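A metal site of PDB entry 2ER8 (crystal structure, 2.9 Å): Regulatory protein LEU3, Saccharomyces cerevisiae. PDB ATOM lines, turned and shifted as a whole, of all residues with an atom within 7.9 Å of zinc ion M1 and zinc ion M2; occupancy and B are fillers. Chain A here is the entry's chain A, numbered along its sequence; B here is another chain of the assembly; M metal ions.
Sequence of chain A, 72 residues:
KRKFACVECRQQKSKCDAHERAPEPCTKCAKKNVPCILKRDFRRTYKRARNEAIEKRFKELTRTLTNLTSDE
The backbone NH of Glu 8 of chain A lies close to the side-chain sulfur of Cys 6 (3.7 Å).
SG of Cys 16 lies close to N of Ala 18, 3.2 Å away.
N of Cys 16 is in hydrogen-bond range of OP2 of DC 8 of chain B (3.1 Å).
N of Ser 14 sits at hydrogen-bond distance from O of Cys 9 (2.9 Å).
The backbone carbonyl oxygen (O) of Cys 29 sits at hydrogen-bond distance from the backbone NH (N) of Val 34 (2.9 Å).
Within 4 Å of zinc ion M1: Cys 6, Cys 26, Cys 29 and Cys 36.
The nearest printed residue that does not touch zinc ion M1 is Cys 9 (4.6 Å).
Four residues have an atom within 4 Å of zinc ion M2: Cys 6, Cys 9, Cys 16 and Cys 26.
Zinc ion M1 is bound by SG of Cys 29 (2.1 Å), SG of Cys 36 (2.3 Å), SG of Cys 26 (2.4 Å) and SG of Cys 6 (2.4 Å).
Zinc ion M1 has four donor atoms within binding distance.
Zinc ion M2 is bound by SG of Cys 26 (2.4 Å), SG of Cys 9 (2.4 Å), SG of Cys 16 (2.5 Å) and SG of Cys 6 (2.6 Å).
Zinc ion M2 has four donor atoms within binding distance.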
ATOM      1  N   PHE A   4      -9.163  19.120 -11.632  1.00  0.00           N
ATOM      2  CA  PHE A   4      -8.114  19.348 -10.632  1.00  0.00           C
ATOM      3  C   PHE A   4      -6.694  19.044 -11.159  1.00  0.00           C
ATOM      4  O   PHE A   4      -6.537  18.238 -12.074  1.00  0.00           O
ATOM      5  CB  PHE A   4      -8.427  18.563  -9.334  1.00  0.00           C
ATOM      6  CG  PHE A   4      -8.278  17.061  -9.459  1.00  0.00           C
ATOM      7  CD1 PHE A   4      -7.737  16.317  -8.395  1.00  0.00           C
ATOM      8  CD2 PHE A   4      -8.699  16.390 -10.608  1.00  0.00           C
ATOM      9  CE1 PHE A   4      -7.608  14.943  -8.477  1.00  0.00           C
ATOM     10  CE2 PHE A   4      -8.579  15.012 -10.704  1.00  0.00           C
ATOM     11  CZ  PHE A   4      -8.030  14.273  -9.625  1.00  0.00           C
ATOM     12  N   ALA A   5      -5.667  19.700 -10.604  1.00  0.00           N
ATOM     13  CA  ALA A   5      -4.273  19.486 -11.003  1.00  0.00           C
ATOM     14  C   ALA A   5      -3.655  18.290 -10.253  1.00  0.00           C
ATOM     15  O   ALA A   5      -4.088  17.884  -9.153  1.00  0.00           O
ATOM     16  CB  ALA A   5      -3.484  20.725 -10.734  1.00  0.00           C
ATOM     17  N   CYS A   6      -2.622  17.696 -10.856  1.00  0.00           N
ATOM     18  CA  CYS A   6      -1.993  16.541 -10.276  1.00  0.00           C
ATOM     19  C   CYS A   6      -1.145  16.972  -9.106  1.00  0.00           C
ATOM     20  O   CYS A   6      -0.711  18.114  -9.017  1.00  0.00           O
ATOM     21  CB  CYS A   6      -1.100  15.855 -11.293  1.00  0.00           C
ATOM     22  SG  CYS A   6       0.432  16.676 -11.428  1.00  0.00           S
ATOM     23  N   VAL A   7      -0.927  16.024  -8.203  1.00  0.00           N
ATOM     24  CA  VAL A   7      -0.147  16.260  -7.013  1.00  0.00           C
ATOM     25  C   VAL A   7       1.045  17.150  -7.214  1.00  0.00           C
ATOM     26  O   VAL A   7       1.122  18.202  -6.637  1.00  0.00           O
ATOM     27  CB  VAL A   7       0.362  14.958  -6.470  1.00  0.00           C
ATOM     28  CG1 VAL A   7       1.119  15.179  -5.202  1.00  0.00           C
ATOM     29  CG2 VAL A   7      -0.809  14.030  -6.261  1.00  0.00           C
ATOM     30  N   GLU A   8       1.988  16.695  -8.028  1.00  0.00           N
ATOM     31  CA  GLU A   8       3.204  17.449  -8.278  1.00  0.00           C
ATOM     32  C   GLU A   8       2.948  18.863  -8.728  1.00  0.00           C
ATOM     33  O   GLU A   8       3.584  19.785  -8.230  1.00  0.00           O
ATOM     34  CB  GLU A   8       4.073  16.745  -9.316  1.00  0.00           C
ATOM     35  CG  GLU A   8       5.454  17.337  -9.444  1.00  0.00           C
ATOM     36  CD  GLU A   8       6.123  17.587  -8.083  1.00  0.00           C
ATOM     37  OE1 GLU A   8       5.893  16.792  -7.147  1.00  0.00           O
ATOM     38  OE2 GLU A   8       6.892  18.574  -7.938  1.00  0.00           O
ATOM     39  N   CYS A   9       2.024  19.072  -9.661  1.00  0.00           N
ATOM     40  CA  CYS A   9       1.750  20.433 -10.084  1.00  0.00           C
ATOM     41  C   CYS A   9       1.182  21.267  -8.970  1.00  0.00           C
ATOM     42  O   CYS A   9       1.499  22.439  -8.856  1.00  0.00           O
ATOM     43  CB  CYS A   9       0.839  20.421 -11.271  1.00  0.00           C
ATOM     44  SG  CYS A   9       1.853  19.859 -12.586  1.00  0.00           S
ATOM     45  N   ARG A  10       0.368  20.656  -8.109  1.00  0.00           N
ATOM     46  CA  ARG A  10      -0.168  21.368  -6.938  1.00  0.00           C
ATOM     47  C   ARG A  10       0.927  21.761  -5.964  1.00  0.00           C
ATOM     48  O   ARG A  10       0.933  22.852  -5.422  1.00  0.00           O
ATOM     49  CB  ARG A  10      -1.164  20.521  -6.181  1.00  0.00           C
ATOM     50  CG  ARG A  10      -2.522  20.554  -6.773  1.00  0.00           C
ATOM     51  CD  ARG A  10      -3.497  19.912  -5.863  1.00  0.00           C
ATOM     52  NE  ARG A  10      -4.837  20.111  -6.391  1.00  0.00           N
ATOM     53  CZ  ARG A  10      -5.909  19.537  -5.862  1.00  0.00           C
ATOM     54  NH1 ARG A  10      -5.772  18.749  -4.811  1.00  0.00           N
ATOM     55  NH2 ARG A  10      -7.103  19.746  -6.402  1.00  0.00           N
ATOM     56  N   SER A  14       2.240  24.837 -10.213  1.00  0.00           N
ATOM     57  CA  SER A  14       2.493  24.989 -11.651  1.00  0.00           C
ATOM     58  C   SER A  14       1.284  24.567 -12.520  1.00  0.00           C
ATOM     59  O   SER A  14       0.434  23.734 -12.092  1.00  0.00           O
ATOM     60  CB  SER A  14       3.729  24.156 -12.044  1.00  0.00           C
ATOM     61  OG  SER A  14       3.479  22.768 -11.924  1.00  0.00           O
ATOM     62  N   LYS A  15       1.201  25.144 -13.713  1.00  0.00           N
ATOM     63  CA  LYS A  15       0.120  24.791 -14.613  1.00  0.00           C
ATOM     64  C   LYS A  15       0.202  23.285 -14.940  1.00  0.00           C
ATOM     65  O   LYS A  15       1.233  22.762 -15.395  1.00  0.00           O
ATOM     66  CB  LYS A  15       0.189  25.582 -15.898  1.00  0.00           C
ATOM     67  CG  LYS A  15      -0.981  25.279 -16.787  1.00  0.00           C
ATOM     68  CD  LYS A  15      -0.753  25.808 -18.166  1.00  0.00           C
ATOM     69  CE  LYS A  15      -1.840  25.302 -19.073  1.00  0.00           C
ATOM     70  NZ  LYS A  15      -3.154  25.533 -18.416  1.00  0.00           N
ATOM     71  N   CYS A  16      -0.911  22.602 -14.666  1.00  0.00           N
ATOM     72  CA  CYS A  16      -1.006  21.173 -14.903  1.00  0.00           C
ATOM     73  C   CYS A  16      -2.033  20.893 -15.980  1.00  0.00           C
ATOM     74  O   CYS A  16      -3.145  21.409 -15.936  1.00  0.00           O
ATOM     75  CB  CYS A  16      -1.390  20.455 -13.623  1.00  0.00           C
ATOM     76  SG  CYS A  16      -2.010  18.823 -13.858  1.00  0.00           S
ATOM     77  N   ASP A  17      -1.652  20.085 -16.940  1.00  0.00           N
ATOM     78  CA  ASP A  17      -2.537  19.718 -18.022  1.00  0.00           C
ATOM     79  C   ASP A  17      -2.854  18.216 -17.937  1.00  0.00           C
ATOM     80  O   ASP A  17      -3.352  17.647 -18.894  1.00  0.00           O
ATOM     81  CB  ASP A  17      -1.867  20.024 -19.360  1.00  0.00           C
ATOM     82  CG  ASP A  17      -0.661  19.120 -19.638  1.00  0.00           C
ATOM     83  OD1 ASP A  17      -0.145  18.458 -18.697  1.00  0.00           O
ATOM     84  OD2 ASP A  17      -0.223  19.080 -20.817  1.00  0.00           O
ATOM     85  N   ALA A  18      -2.551  17.586 -16.810  1.00  0.00           N
ATOM     86  CA  ALA A  18      -2.790  16.151 -16.640  1.00  0.00           C
ATOM     87  C   ALA A  18      -4.019  15.693 -17.383  1.00  0.00           C
ATOM     88  O   ALA A  18      -3.952  14.678 -18.078  1.00  0.00           O
ATOM     89  CB  ALA A  18      -2.925  15.808 -15.167  1.00  0.00           C
ATOM     90  N   HIS A  19      -5.119  16.422 -17.254  1.00  0.00           N
ATOM     91  CA  HIS A  19      -6.373  16.056 -17.906  1.00  0.00           C
ATOM     92  C   HIS A  19      -6.259  15.997 -19.423  1.00  0.00           C
ATOM     93  O   HIS A  19      -6.400  14.921 -20.033  1.00  0.00           O
ATOM     94  CB  HIS A  19      -7.482  17.030 -17.518  1.00  0.00           C
ATOM     95  CG  HIS A  19      -7.760  17.055 -16.051  1.00  0.00           C
ATOM     96  ND1 HIS A  19      -8.348  15.990 -15.378  1.00  0.00           N
ATOM     97  CD2 HIS A  19      -7.533  18.006 -15.110  1.00  0.00           C
ATOM     98  CE1 HIS A  19      -8.461  16.282 -14.103  1.00  0.00           C
ATOM     99  NE2 HIS A  19      -7.976  17.503 -13.904  1.00  0.00           N
ATOM    100  N   GLU A  24      -1.176   9.563 -20.468  1.00  0.00           N
ATOM    101  CA  GLU A  24       0.164  10.109 -20.414  1.00  0.00           C
ATOM    102  C   GLU A  24       0.262  11.169 -19.318  1.00  0.00           C
ATOM    103  O   GLU A  24      -0.555  12.088 -19.253  1.00  0.00           O
ATOM    104  CB  GLU A  24       0.527  10.710 -21.774  1.00  0.00           C
ATOM    105  CG  GLU A  24       0.387   9.731 -22.930  1.00  0.00           C
ATOM    106  CD  GLU A  24       1.139   8.431 -22.688  1.00  0.00           C
ATOM    107  OE1 GLU A  24       2.379   8.481 -22.525  1.00  0.00           O
ATOM    108  OE2 GLU A  24       0.496   7.358 -22.640  1.00  0.00           O
ATOM    109  N   PRO A  25       1.268  11.045 -18.423  1.00  0.00           N
ATOM    110  CA  PRO A  25       1.503  11.961 -17.311  1.00  0.00           C
ATOM    111  C   PRO A  25       1.455  13.412 -17.763  1.00  0.00           C
ATOM    112  O   PRO A  25       1.738  13.705 -18.922  1.00  0.00           O
ATOM    113  CB  PRO A  25       2.893  11.564 -16.806  1.00  0.00           C
ATOM    114  CG  PRO A  25       2.873  10.084 -16.991  1.00  0.00           C
ATOM    115  CD  PRO A  25       2.266   9.956 -18.398  1.00  0.00           C
ATOM    116  N   CYS A  26       1.109  14.325 -16.857  1.00  0.00           N
ATOM    117  CA  CYS A  26       1.025  15.737 -17.222  1.00  0.00           C
ATOM    118  C   CYS A  26       2.400  16.156 -17.678  1.00  0.00           C
ATOM    119  O   CYS A  26       3.418  15.619 -17.233  1.00  0.00           O
ATOM    120  CB  CYS A  26       0.567  16.606 -16.049  1.00  0.00           C
ATOM    121  SG  CYS A  26       1.846  16.876 -14.805  1.00  0.00           S
ATOM    122  N   THR A  27       2.405  17.104 -18.612  1.00  0.00           N
ATOM    123  CA  THR A  27       3.626  17.645 -19.184  1.00  0.00           C
ATOM    124  C   THR A  27       4.701  17.803 -18.113  1.00  0.00           C
ATOM    125  O   THR A  27       5.742  17.141 -18.151  1.00  0.00           O
ATOM    126  CB  THR A  27       3.355  19.019 -19.831  1.00  0.00           C
ATOM    127  OG1 THR A  27       2.337  18.897 -20.836  1.00  0.00           O
ATOM    128  CG2 THR A  27       4.608  19.537 -20.460  1.00  0.00           C
ATOM    129  N   LYS A  28       4.423  18.686 -17.151  1.00  0.00           N
ATOM    130  CA  LYS A  28       5.328  18.980 -16.049  1.00  0.00           C
ATOM    131  C   LYS A  28       5.892  17.741 -15.371  1.00  0.00           C
ATOM    132  O   LYS A  28       7.099  17.669 -15.129  1.00  0.00           O
ATOM    133  CB  LYS A  28       4.610  19.846 -15.015  1.00  0.00           C
ATOM    134  CG  LYS A  28       4.388  21.307 -15.425  1.00  0.00           C
ATOM    135  CD  LYS A  28       5.677  22.073 -15.308  1.00  0.00           C
ATOM    136  CE  LYS A  28       5.520  23.545 -15.510  1.00  0.00           C
ATOM    137  NZ  LYS A  28       6.857  24.243 -15.349  1.00  0.00           N
ATOM    138  N   CYS A  29       5.032  16.769 -15.075  1.00  0.00           N
ATOM    139  CA  CYS A  29       5.451  15.523 -14.407  1.00  0.00           C
ATOM    140  C   CYS A  29       6.365  14.660 -15.280  1.00  0.00           C
ATOM    141  O   CYS A  29       7.289  14.012 -14.802  1.00  0.00           O
ATOM    142  CB  CYS A  29       4.244  14.688 -13.957  1.00  0.00           C
ATOM    143  SG  CYS A  29       3.538  15.200 -12.374  1.00  0.00           S
ATOM    144  N   ALA A  30       6.070  14.650 -16.573  1.00  0.00           N
ATOM    145  CA  ALA A  30       6.877  13.916 -17.514  1.00  0.00           C
ATOM    146  C   ALA A  30       8.300  14.521 -17.553  1.00  0.00           C
ATOM    147  O   ALA A  30       9.302  13.819 -17.331  1.00  0.00           O
ATOM    148  CB  ALA A  30       6.236  13.994 -18.883  1.00  0.00           C
ATOM    149  N   VAL A  34       8.723  12.001 -13.283  1.00  0.00           N
ATOM    150  CA  VAL A  34       8.103  11.558 -12.049  1.00  0.00           C
ATOM    151  C   VAL A  34       6.665  11.179 -12.304  1.00  0.00           C
ATOM    152  O   VAL A  34       6.024  11.637 -13.260  1.00  0.00           O
ATOM    153  CB  VAL A  34       8.140  12.646 -10.949  1.00  0.00           C
ATOM    154  CG1 VAL A  34       9.563  12.928 -10.538  1.00  0.00           C
ATOM    155  CG2 VAL A  34       7.480  13.918 -11.456  1.00  0.00           C
ATOM    156  N   PRO A  35       6.128  10.313 -11.438  1.00  0.00           N
ATOM    157  CA  PRO A  35       4.750   9.832 -11.527  1.00  0.00           C
ATOM    158  C   PRO A  35       3.723  10.952 -11.416  1.00  0.00           C
ATOM    159  O   PRO A  35       3.728  11.730 -10.456  1.00  0.00           O
ATOM    160  CB  PRO A  35       4.667   8.843 -10.366  1.00  0.00           C
ATOM    161  CG  PRO A  35       6.058   8.338 -10.256  1.00  0.00           C
ATOM    162  CD  PRO A  35       6.873   9.594 -10.396  1.00  0.00           C
ATOM    163  N   CYS A  36       2.823  11.024 -12.398  1.00  0.00           N
ATOM    164  CA  CYS A  36       1.790  12.040 -12.360  1.00  0.00           C
ATOM    165  C   CYS A  36       0.582  11.481 -11.619  1.00  0.00           C
ATOM    166  O   CYS A  36      -0.311  10.883 -12.223  1.00  0.00           O
ATOM    167  CB  CYS A  36       1.404  12.429 -13.779  1.00  0.00           C
ATOM    168  SG  CYS A  36       0.171  13.692 -13.872  1.00  0.00           S
ATOM    169  N   ILE A  37       0.546  11.682 -10.307  1.00  0.00           N
ATOM    170  CA  ILE A  37      -0.541  11.161  -9.506  1.00  0.00           C
ATOM    171  C   ILE A  37      -1.632  12.176  -9.251  1.00  0.00           C
ATOM    172  O   ILE A  37      -1.340  13.350  -9.083  1.00  0.00           O
ATOM    173  CB  ILE A  37       0.004  10.683  -8.170  1.00  0.00           C
ATOM    174  CG1 ILE A  37       1.083   9.635  -8.422  1.00  0.00           C
ATOM    175  CG2 ILE A  37      -1.111  10.106  -7.344  1.00  0.00           C
ATOM    176  CD1 ILE A  37       1.737   9.066  -7.189  1.00  0.00           C
ATOM    177  N   LEU A  38      -2.894  11.739  -9.239  1.00  0.00           N
ATOM    178  CA  LEU A  38      -4.019  12.647  -8.944  1.00  0.00           C
ATOM    179  C   LEU A  38      -4.700  12.309  -7.603  1.00  0.00           C
ATOM    180  O   LEU A  38      -5.051  11.154  -7.357  1.00  0.00           O
ATOM    181  CB  LEU A  38      -5.072  12.601 -10.050  1.00  0.00           C
ATOM    182  CG  LEU A  38      -4.574  12.532 -11.491  1.00  0.00           C
ATOM    183  CD1 LEU A  38      -5.602  13.153 -12.416  1.00  0.00           C
ATOM    184  CD2 LEU A  38      -3.276  13.268 -11.642  1.00  0.00           C
ATOM    185  P    DC B   8      -4.077  25.142 -14.269  1.00  0.00           P
ATOM    186  OP1  DC B   8      -4.429  24.682 -15.648  1.00  0.00           O
ATOM    187  OP2  DC B   8      -3.151  24.350 -13.389  1.00  0.00           O
ATOM    188  O5'  DC B   8      -3.477  26.594 -14.427  1.00  0.00           O
ATOM    189  C5'  DC B   8      -3.682  27.491 -13.380  1.00  0.00           C
ATOM    190  C4'  DC B   8      -2.900  28.742 -13.617  1.00  0.00           C
ATOM    191  O4'  DC B   8      -2.794  29.423 -12.357  1.00  0.00           O
ATOM    192  C3'  DC B   8      -1.465  28.472 -14.060  1.00  0.00           C
ATOM    193  O3'  DC B   8      -1.115  29.573 -14.896  1.00  0.00           O
ATOM    194  C2'  DC B   8      -0.733  28.347 -12.724  1.00  0.00           C
ATOM    195  C1'  DC B   8      -1.487  29.334 -11.834  1.00  0.00           C
ATOM    196  N1   DC B   8      -1.608  28.987 -10.403  1.00  0.00           N
ATOM    197  C2   DC B   8      -1.696  30.020  -9.498  1.00  0.00           C
ATOM    198  O2   DC B   8      -1.741  31.182  -9.944  1.00  0.00           O
ATOM    199  N3   DC B   8      -1.748  29.749  -8.170  1.00  0.00           N
ATOM    200  C4   DC B   8      -1.721  28.481  -7.747  1.00  0.00           C
ATOM    201  N4   DC B   8      -1.760  28.273  -6.426  1.00  0.00           N
ATOM    202  C5   DC B   8      -1.668  27.392  -8.663  1.00  0.00           C
ATOM    203  C6   DC B   8      -1.603  27.683  -9.977  1.00  0.00           C
HETATM  204 ZN    ZN M   1       1.531  15.328 -13.059  1.00  0.00          ZN
HETATM  205 ZN    ZN M   2       0.365  18.190 -13.503  1.00  0.00          ZN
